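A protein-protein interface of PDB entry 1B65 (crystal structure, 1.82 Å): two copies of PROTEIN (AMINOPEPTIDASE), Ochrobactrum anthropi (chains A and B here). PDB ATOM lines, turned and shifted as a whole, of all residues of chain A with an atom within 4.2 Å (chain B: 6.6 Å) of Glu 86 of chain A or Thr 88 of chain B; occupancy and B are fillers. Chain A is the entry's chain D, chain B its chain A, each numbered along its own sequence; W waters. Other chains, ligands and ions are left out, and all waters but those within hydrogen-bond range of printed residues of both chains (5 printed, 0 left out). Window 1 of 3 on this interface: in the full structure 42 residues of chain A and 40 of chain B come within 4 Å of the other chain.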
ATOM      1  N   GLY A  85     -18.661 -10.550 -14.258  1.00  0.00           N
ATOM      2  CA  GLY A  85     -18.824  -9.506 -13.250  1.00  0.00           C
ATOM      3  C   GLY A  85     -17.759  -8.424 -13.544  1.00  0.00           C
ATOM      4  O   GLY A  85     -16.995  -8.572 -14.487  1.00  0.00           O
ATOM      5  N   GLU A  86     -17.813  -7.383 -12.739  1.00  0.00           N
ATOM      6  CA  GLU A  86     -16.865  -6.286 -12.985  1.00  0.00           C
ATOM      7  C   GLU A  86     -15.938  -6.012 -11.819  1.00  0.00           C
ATOM      8  O   GLU A  86     -16.316  -6.131 -10.658  1.00  0.00           O
ATOM      9  CB  GLU A  86     -17.698  -5.032 -13.335  1.00  0.00           C
ATOM     10  CG  GLU A  86     -16.887  -3.745 -13.572  1.00  0.00           C
ATOM     11  CD  GLU A  86     -16.006  -3.993 -14.801  1.00  0.00           C
ATOM     12  OE1 GLU A  86     -14.902  -4.548 -14.685  1.00  0.00           O
ATOM     13  OE2 GLU A  86     -16.459  -3.692 -15.916  1.00  0.00           O
ATOM     14  N   MET A  87     -14.672  -5.735 -12.198  1.00  0.00           N
ATOM     15  CA  MET A  87     -13.721  -5.248 -11.201  1.00  0.00           C
ATOM     16  C   MET A  87     -12.901  -4.217 -11.992  1.00  0.00           C
ATOM     17  O   MET A  87     -12.164  -4.687 -12.864  1.00  0.00           O
ATOM     18  CB  MET A  87     -12.821  -6.321 -10.588  1.00  0.00           C
ATOM     19  CG  MET A  87     -11.779  -5.705  -9.656  1.00  0.00           C
ATOM     20  SD  MET A  87     -10.706  -6.918  -8.877  1.00  0.00           S
ATOM     21  CE  MET A  87     -11.796  -7.658  -7.657  1.00  0.00           C
ATOM     22  N   THR A  88     -13.015  -2.943 -11.725  1.00  0.00           N
ATOM     23  CA  THR A  88     -12.237  -1.954 -12.487  1.00  0.00           C
ATOM     24  C   THR A  88     -10.812  -1.826 -11.937  1.00  0.00           C
ATOM     25  O   THR A  88     -10.446  -2.396 -10.907  1.00  0.00           O
ATOM     26  CB  THR A  88     -12.880  -0.547 -12.403  1.00  0.00           C
ATOM     27  OG1 THR A  88     -12.817  -0.052 -11.041  1.00  0.00           O
ATOM     28  CG2 THR A  88     -14.339  -0.598 -12.863  1.00  0.00           C
ATOM     29  N   ILE A 111     -21.569   0.314  -9.919  1.00  0.00           N
ATOM     30  CA  ILE A 111     -20.144   0.490 -10.265  1.00  0.00           C
ATOM     31  C   ILE A 111     -19.821   1.934 -10.644  1.00  0.00           C
ATOM     32  O   ILE A 111     -18.817   2.510 -10.233  1.00  0.00           O
ATOM     33  CB  ILE A 111     -19.768  -0.453 -11.415  1.00  0.00           C
ATOM     34  CG1 ILE A 111     -19.689  -1.912 -10.967  1.00  0.00           C
ATOM     35  CG2 ILE A 111     -18.478  -0.009 -12.131  1.00  0.00           C
ATOM     36  CD1 ILE A 111     -18.478  -2.383 -10.176  1.00  0.00           C
ATOM     37  N   VAL A 142     -12.949  -0.880  -8.328  1.00  0.00           N
ATOM     38  CA  VAL A 142     -14.348  -0.932  -7.866  1.00  0.00           C
ATOM     39  C   VAL A 142     -14.939  -2.240  -8.392  1.00  0.00           C
ATOM     40  O   VAL A 142     -14.811  -2.532  -9.594  1.00  0.00           O
ATOM     41  CB  VAL A 142     -15.125   0.272  -8.436  1.00  0.00           C
ATOM     42  CG1 VAL A 142     -16.588   0.231  -8.030  1.00  0.00           C
ATOM     43  CG2 VAL A 142     -14.507   1.598  -8.006  1.00  0.00           C
ATOM     44  N   ALA A 143     -15.551  -3.033  -7.509  1.00  0.00           N
ATOM     45  CA  ALA A 143     -16.052  -4.342  -7.901  1.00  0.00           C
ATOM     46  C   ALA A 143     -17.485  -4.521  -7.424  1.00  0.00           C
ATOM     47  O   ALA A 143     -18.025  -3.640  -6.734  1.00  0.00           O
ATOM     48  CB  ALA A 143     -15.168  -5.446  -7.289  1.00  0.00           C
ATOM     49  N   GLU A 144     -18.077  -5.629  -7.858  1.00  0.00           N
ATOM     50  CA  GLU A 144     -19.486  -5.839  -7.522  1.00  0.00           C
ATOM     51  C   GLU A 144     -19.903  -7.295  -7.498  1.00  0.00           C
ATOM     52  O   GLU A 144     -19.224  -8.175  -8.048  1.00  0.00           O
ATOM     53  CB  GLU A 144     -20.324  -5.173  -8.642  1.00  0.00           C
ATOM     54  CG  GLU A 144     -20.043  -5.627 -10.069  1.00  0.00           C
ATOM     55  CD  GLU A 144     -20.714  -6.897 -10.514  1.00  0.00           C
ATOM     56  OE1 GLU A 144     -21.616  -7.448  -9.817  1.00  0.00           O
ATOM     57  OE2 GLU A 144     -20.310  -7.465 -11.571  1.00  0.00           O
ATOM     58  N   GLU B  86      -7.983   2.889 -18.478  1.00  0.00           N
ATOM     59  CA  GLU B  86      -9.144   2.071 -18.138  1.00  0.00           C
ATOM     60  C   GLU B  86      -9.988   1.731 -19.351  1.00  0.00           C
ATOM     61  O   GLU B  86     -10.182   2.558 -20.247  1.00  0.00           O
ATOM     62  CB  GLU B  86      -9.973   2.813 -17.074  1.00  0.00           C
ATOM     63  CG  GLU B  86     -11.210   2.032 -16.605  1.00  0.00           C
ATOM     64  CD  GLU B  86     -10.768   0.703 -15.954  1.00  0.00           C
ATOM     65  OE1 GLU B  86     -10.468   0.705 -14.741  1.00  0.00           O
ATOM     66  OE2 GLU B  86     -10.630  -0.310 -16.657  1.00  0.00           O
ATOM     67  N   MET B  87     -10.492   0.506 -19.335  1.00  0.00           N
ATOM     68  CA  MET B  87     -11.493   0.047 -20.292  1.00  0.00           C
ATOM     69  C   MET B  87     -12.324  -0.964 -19.485  1.00  0.00           C
ATOM     70  O   MET B  87     -11.800  -2.058 -19.233  1.00  0.00           O
ATOM     71  CB  MET B  87     -10.973  -0.604 -21.586  1.00  0.00           C
ATOM     72  CG  MET B  87     -12.141  -1.127 -22.439  1.00  0.00           C
ATOM     73  SD  MET B  87     -11.542  -1.912 -23.967  1.00  0.00           S
ATOM     74  CE  MET B  87     -10.942  -0.458 -24.852  1.00  0.00           C
ATOM     75  N   THR B  88     -13.534  -0.590 -19.110  1.00  0.00           N
ATOM     76  CA  THR B  88     -14.378  -1.538 -18.375  1.00  0.00           C
ATOM     77  C   THR B  88     -15.037  -2.569 -19.265  1.00  0.00           C
ATOM     78  O   THR B  88     -14.970  -2.526 -20.499  1.00  0.00           O
ATOM     79  CB  THR B  88     -15.465  -0.762 -17.594  1.00  0.00           C
ATOM     80  OG1 THR B  88     -16.458  -0.262 -18.507  1.00  0.00           O
ATOM     81  CG2 THR B  88     -14.848   0.387 -16.774  1.00  0.00           C
ATOM     82  N   GLY B  89     -15.675  -3.568 -18.627  1.00  0.00           N
ATOM     83  CA  GLY B  89     -16.405  -4.619 -19.293  1.00  0.00           C
ATOM     84  C   GLY B  89     -15.568  -5.727 -19.924  1.00  0.00           C
ATOM     85  O   GLY B  89     -16.116  -6.604 -20.605  1.00  0.00           O
ATOM     86  N   THR B  90     -14.260  -5.781 -19.635  1.00  0.00           N
ATOM     87  CA  THR B  90     -13.470  -6.767 -20.375  1.00  0.00           C
ATOM     88  C   THR B  90     -13.400  -8.136 -19.744  1.00  0.00           C
ATOM     89  O   THR B  90     -13.032  -9.060 -20.492  1.00  0.00           O
ATOM     90  CB  THR B  90     -12.029  -6.238 -20.583  1.00  0.00           C
ATOM     91  OG1 THR B  90     -11.400  -6.226 -19.296  1.00  0.00           O
ATOM     92  CG2 THR B  90     -12.090  -4.820 -21.165  1.00  0.00           C
ATOM     93  N   HIS B  91     -13.777  -8.294 -18.462  1.00  0.00           N
ATOM     94  CA  HIS B  91     -13.706  -9.621 -17.859  1.00  0.00           C
ATOM     95  C   HIS B  91     -14.636 -10.602 -18.582  1.00  0.00           C
ATOM     96  O   HIS B  91     -14.214 -11.715 -18.822  1.00  0.00           O
ATOM     97  CB  HIS B  91     -14.039  -9.590 -16.346  1.00  0.00           C
ATOM     98  CG  HIS B  91     -13.101  -8.673 -15.622  1.00  0.00           C
ATOM     99  ND1 HIS B  91     -11.726  -8.837 -15.678  1.00  0.00           N
ATOM    100  CD2 HIS B  91     -13.330  -7.599 -14.822  1.00  0.00           C
ATOM    101  CE1 HIS B  91     -11.137  -7.890 -14.943  1.00  0.00           C
ATOM    102  NE2 HIS B  91     -12.095  -7.111 -14.425  1.00  0.00           N
ATOM    103  N   ILE B  93     -15.815 -10.136 -21.620  1.00  0.00           N
ATOM    104  CA  ILE B  93     -15.330 -10.271 -23.019  1.00  0.00           C
ATOM    105  C   ILE B  93     -14.316 -11.412 -23.049  1.00  0.00           C
ATOM    106  O   ILE B  93     -14.309 -12.238 -23.925  1.00  0.00           O
ATOM    107  CB  ILE B  93     -14.702  -8.959 -23.522  1.00  0.00           C
ATOM    108  CG1 ILE B  93     -15.888  -7.984 -23.791  1.00  0.00           C
ATOM    109  CG2 ILE B  93     -13.950  -9.217 -24.826  1.00  0.00           C
ATOM    110  CD1 ILE B  93     -15.312  -6.559 -24.025  1.00  0.00           C
ATOM    111  N   ILE B 111     -15.013   8.195 -16.475  1.00  0.00           N
ATOM    112  CA  ILE B 111     -15.425   6.775 -16.566  1.00  0.00           C
ATOM    113  C   ILE B 111     -16.651   6.477 -15.731  1.00  0.00           C
ATOM    114  O   ILE B 111     -17.537   5.778 -16.192  1.00  0.00           O
ATOM    115  CB  ILE B 111     -14.291   5.871 -16.035  1.00  0.00           C
ATOM    116  CG1 ILE B 111     -13.111   5.840 -16.998  1.00  0.00           C
ATOM    117  CG2 ILE B 111     -14.776   4.439 -15.715  1.00  0.00           C
ATOM    118  CD1 ILE B 111     -13.328   5.039 -18.295  1.00  0.00           C
ATOM    119  N   HIS B 115     -20.149   5.281 -17.145  1.00  0.00           N
ATOM    120  CA  HIS B 115     -20.633   3.916 -16.854  1.00  0.00           C
ATOM    121  C   HIS B 115     -22.036   3.974 -16.257  1.00  0.00           C
ATOM    122  O   HIS B 115     -22.944   3.268 -16.704  1.00  0.00           O
ATOM    123  CB  HIS B 115     -19.647   3.248 -15.889  1.00  0.00           C
ATOM    124  CG  HIS B 115     -19.834   1.770 -15.726  1.00  0.00           C
ATOM    125  ND1 HIS B 115     -20.857   1.227 -15.017  1.00  0.00           N
ATOM    126  CD2 HIS B 115     -19.078   0.734 -16.190  1.00  0.00           C
ATOM    127  CE1 HIS B 115     -20.775  -0.107 -15.036  1.00  0.00           C
ATOM    128  NE2 HIS B 115     -19.713  -0.405 -15.773  1.00  0.00           N
ATOM    129  N   MET B 139     -22.939  -4.885 -18.054  1.00  0.00           N
ATOM    130  CA  MET B 139     -21.526  -4.531 -17.779  1.00  0.00           C
ATOM    131  C   MET B 139     -20.965  -3.840 -19.028  1.00  0.00           C
ATOM    132  O   MET B 139     -20.394  -4.487 -19.912  1.00  0.00           O
ATOM    133  CB  MET B 139     -20.769  -5.826 -17.505  1.00  0.00           C
ATOM    134  CG  MET B 139     -21.111  -6.458 -16.146  1.00  0.00           C
ATOM    135  SD  MET B 139     -20.434  -8.117 -15.961  1.00  0.00           S
ATOM    136  CE  MET B 139     -20.908  -8.975 -17.422  1.00  0.00           C
ATOM    137  N   PRO B 140     -21.179  -2.543 -19.131  1.00  0.00           N
ATOM    138  CA  PRO B 140     -20.773  -1.798 -20.315  1.00  0.00           C
ATOM    139  C   PRO B 140     -19.279  -1.641 -20.493  1.00  0.00           C
ATOM    140  O   PRO B 140     -18.505  -1.739 -19.553  1.00  0.00           O
ATOM    141  CB  PRO B 140     -21.416  -0.433 -20.181  1.00  0.00           C
ATOM    142  CG  PRO B 140     -21.949  -0.340 -18.800  1.00  0.00           C
ATOM    143  CD  PRO B 140     -21.875  -1.695 -18.147  1.00  0.00           C
ATOM    144  N   VAL B 141     -18.912  -1.353 -21.730  1.00  0.00           N
ATOM    145  CA  VAL B 141     -17.504  -1.152 -22.099  1.00  0.00           C
ATOM    146  C   VAL B 141     -17.301   0.366 -22.195  1.00  0.00           C
ATOM    147  O   VAL B 141     -17.819   0.999 -23.119  1.00  0.00           O
ATOM    148  CB  VAL B 141     -17.148  -1.780 -23.446  1.00  0.00           C
ATOM    149  CG1 VAL B 141     -15.644  -1.574 -23.754  1.00  0.00           C
ATOM    150  CG2 VAL B 141     -17.375  -3.299 -23.433  1.00  0.00           C
ATOM    151  N   VAL B 142     -16.607   0.905 -21.204  1.00  0.00           N
ATOM    152  CA  VAL B 142     -16.336   2.344 -21.108  1.00  0.00           C
ATOM    153  C   VAL B 142     -14.824   2.525 -20.999  1.00  0.00           C
ATOM    154  O   VAL B 142     -14.200   1.905 -20.126  1.00  0.00           O
ATOM    155  CB  VAL B 142     -17.040   2.976 -19.896  1.00  0.00           C
ATOM    156  CG1 VAL B 142     -16.875   4.492 -19.871  1.00  0.00           C
ATOM    157  CG2 VAL B 142     -18.529   2.601 -19.876  1.00  0.00           C
ATOM    158  N   ALA B 143     -14.271   3.383 -21.842  1.00  0.00           N
ATOM    159  CA  ALA B 143     -12.817   3.537 -21.889  1.00  0.00           C
ATOM    160  C   ALA B 143     -12.430   5.014 -21.918  1.00  0.00           C
ATOM    161  O   ALA B 143     -13.332   5.856 -21.976  1.00  0.00           O
ATOM    162  CB  ALA B 143     -12.355   2.860 -23.196  1.00  0.00           C
ATOM    163  N   ILE B 293      -9.779  -2.884 -28.764  1.00  0.00           N
ATOM    164  CA  ILE B 293     -10.885  -3.849 -28.684  1.00  0.00           C
ATOM    165  C   ILE B 293     -11.331  -4.110 -30.115  1.00  0.00           C
ATOM    166  O   ILE B 293     -11.348  -3.151 -30.891  1.00  0.00           O
ATOM    167  CB  ILE B 293     -12.022  -3.351 -27.787  1.00  0.00           C
ATOM    168  CG1 ILE B 293     -13.139  -4.399 -27.778  1.00  0.00           C
ATOM    169  CG2 ILE B 293     -12.493  -1.946 -28.175  1.00  0.00           C
ATOM    170  CD1 ILE B 293     -14.216  -4.038 -26.727  1.00  0.00           C
HETATM  171  O   HOH W   1     -17.369  -7.874 -17.552  1.00  0.00           O
HETATM  172  O   HOH W   2     -15.463  -6.552 -16.774  1.00  0.00           O
HETATM  173  O   HOH W   3     -12.924  -4.636 -17.213  1.00  0.00           O
HETATM  174  O   HOH W   4     -22.155  -9.067 -12.941  1.00  0.00           O
HETATM  175  O   HOH W   5     -18.791  -2.849 -16.860  1.00  0.00           O
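Glu 86 of chain A touches Thr 88 of chain B, and with the chains exchanged Thr 88 of chain A touches Glu 86 of chain B. Positions printed for both chains: 86, 87, 88, 111, 142 and 143.
Among the printed residues, pairs that only touch across the chains: Glu 86 of chain A with His 91 of chain B, Glu 86 of chain A with Thr 88 of chain B, Thr 88 of chain A with Glu 86 of chain B, Gly 85 of chain A with His 91 of chain B and Ile 111 of chain A with His 115 of chain B.
OG1 of Thr 88 of chain B lies within hydrogen-bond range of O of Pro 140 of chain B (2.7 Å). The backbone NH of Thr 88 of chain B is in hydrogen-bond range of the backbone carbonyl oxygen of Val 142 of chain B, 2.8 Å away. The backbone carbonyl oxygen of Pro 140 of chain B sits at hydrogen-bond distance from the backbone NH of Gly 89 of chain B, at 3.5 Å. The backbone NH (N) of Glu 86 of chain A sits at hydrogen-bond distance from the side-chain carboxylate (OE2) of Glu 144 of chain A (2.8 Å). The backbone NH of Thr 88 of chain A is in hydrogen-bond range of the backbone carbonyl oxygen of Val 142 of chain A.
Water W5 lies within hydrogen-bond range of the side-chain carboxylate of Glu 86 of chain A (2.7 Å), a ring nitrogen (NE2) of His 115 of chain B (2.8 Å) and the backbone carbonyl oxygen of Pro 140 of chain B (2.9 Å). Water W4 lies within hydrogen-bond range of the side-chain carboxylate (OE2) of Glu 144 of chain A (2.8 Å) and the side-chain sulfur (SD) of Met 139 of chain B (3.6 Å). Water W2 lies within hydrogen-bond range of OE1 of Glu 86 of chain A (2.9 Å), N of His 91 of chain B (3.0 Å), N of Thr 90 of chain B (3.2 Å) and O of Gly 85 of chain A (3.4 Å). Water W3 lies within hydrogen-bond range of N of Thr 90 of chain B, OE1 of Glu 86 of chain A, N of Gly 89 of chain B and O of Met 87 of chain B. Water W1 bridges the backbone carbonyl oxygen of Gly 85 of chain A and the side-chain sulfur of Met 139 of chain B.
Glu 86 of chain A touches just these residues of chain B: Thr 88, Gly 89 and His 91. Of the printed residues of chain B, Ile 111 of chain A touches His 115. Of chain A, only Glu 86 comes within 4 Å of Thr 88 of chain B. Of the printed residues of chain A, Gly 89 of chain B touches Glu 86. Printed residues of chain A within 4 Å of His 115 of chain B: Ile 111. Ala 143 of chain B touches none of the printed residues of chain A. The nearest residue of chain B that does not touch Glu 86 of chain A is Met 139 of chain B (4.2 Å). The nearest residue of chain A that does not touch Thr 88 of chain B is Thr 88 of chain A (4.1 Å). The nearest printed residue of chain B that does not touch Met 87 of chain A is Glu 86 of chain B (6.0 Å).
The backbone NH (N) of Gly 89 of chain B sits at hydrogen-bond distance from the side-chain carboxylate (OE2) of Glu 86 of chain A, at 2.8 Å. A ring nitrogen (NE2) of His 91 of chain B is in hydrogen-bond range of the backbone carbonyl oxygen of Met 87 of chain A (2.9 Å). The backbone NH (N) of Gly 85 of chain A lies close to the side-chain sulfur (SD) of Met 139 of chain B, at 3.5 Å.
Printed residues of chain B that touch a printed residue of chain A: Glu 86, Thr 88, Gly 89, His 91, His 115 and Met 139. Hydrophobic or aromatic side chains of chain B that line the printed part of chain A: His 91, His 115 and Met 139. Among the printed residues, 8 pairs touch across the chains. Among the printed residues, no Asp or Glu carboxylate lies within 4 Å of a Lys or Arg side-chain nitrogen of the other chain.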
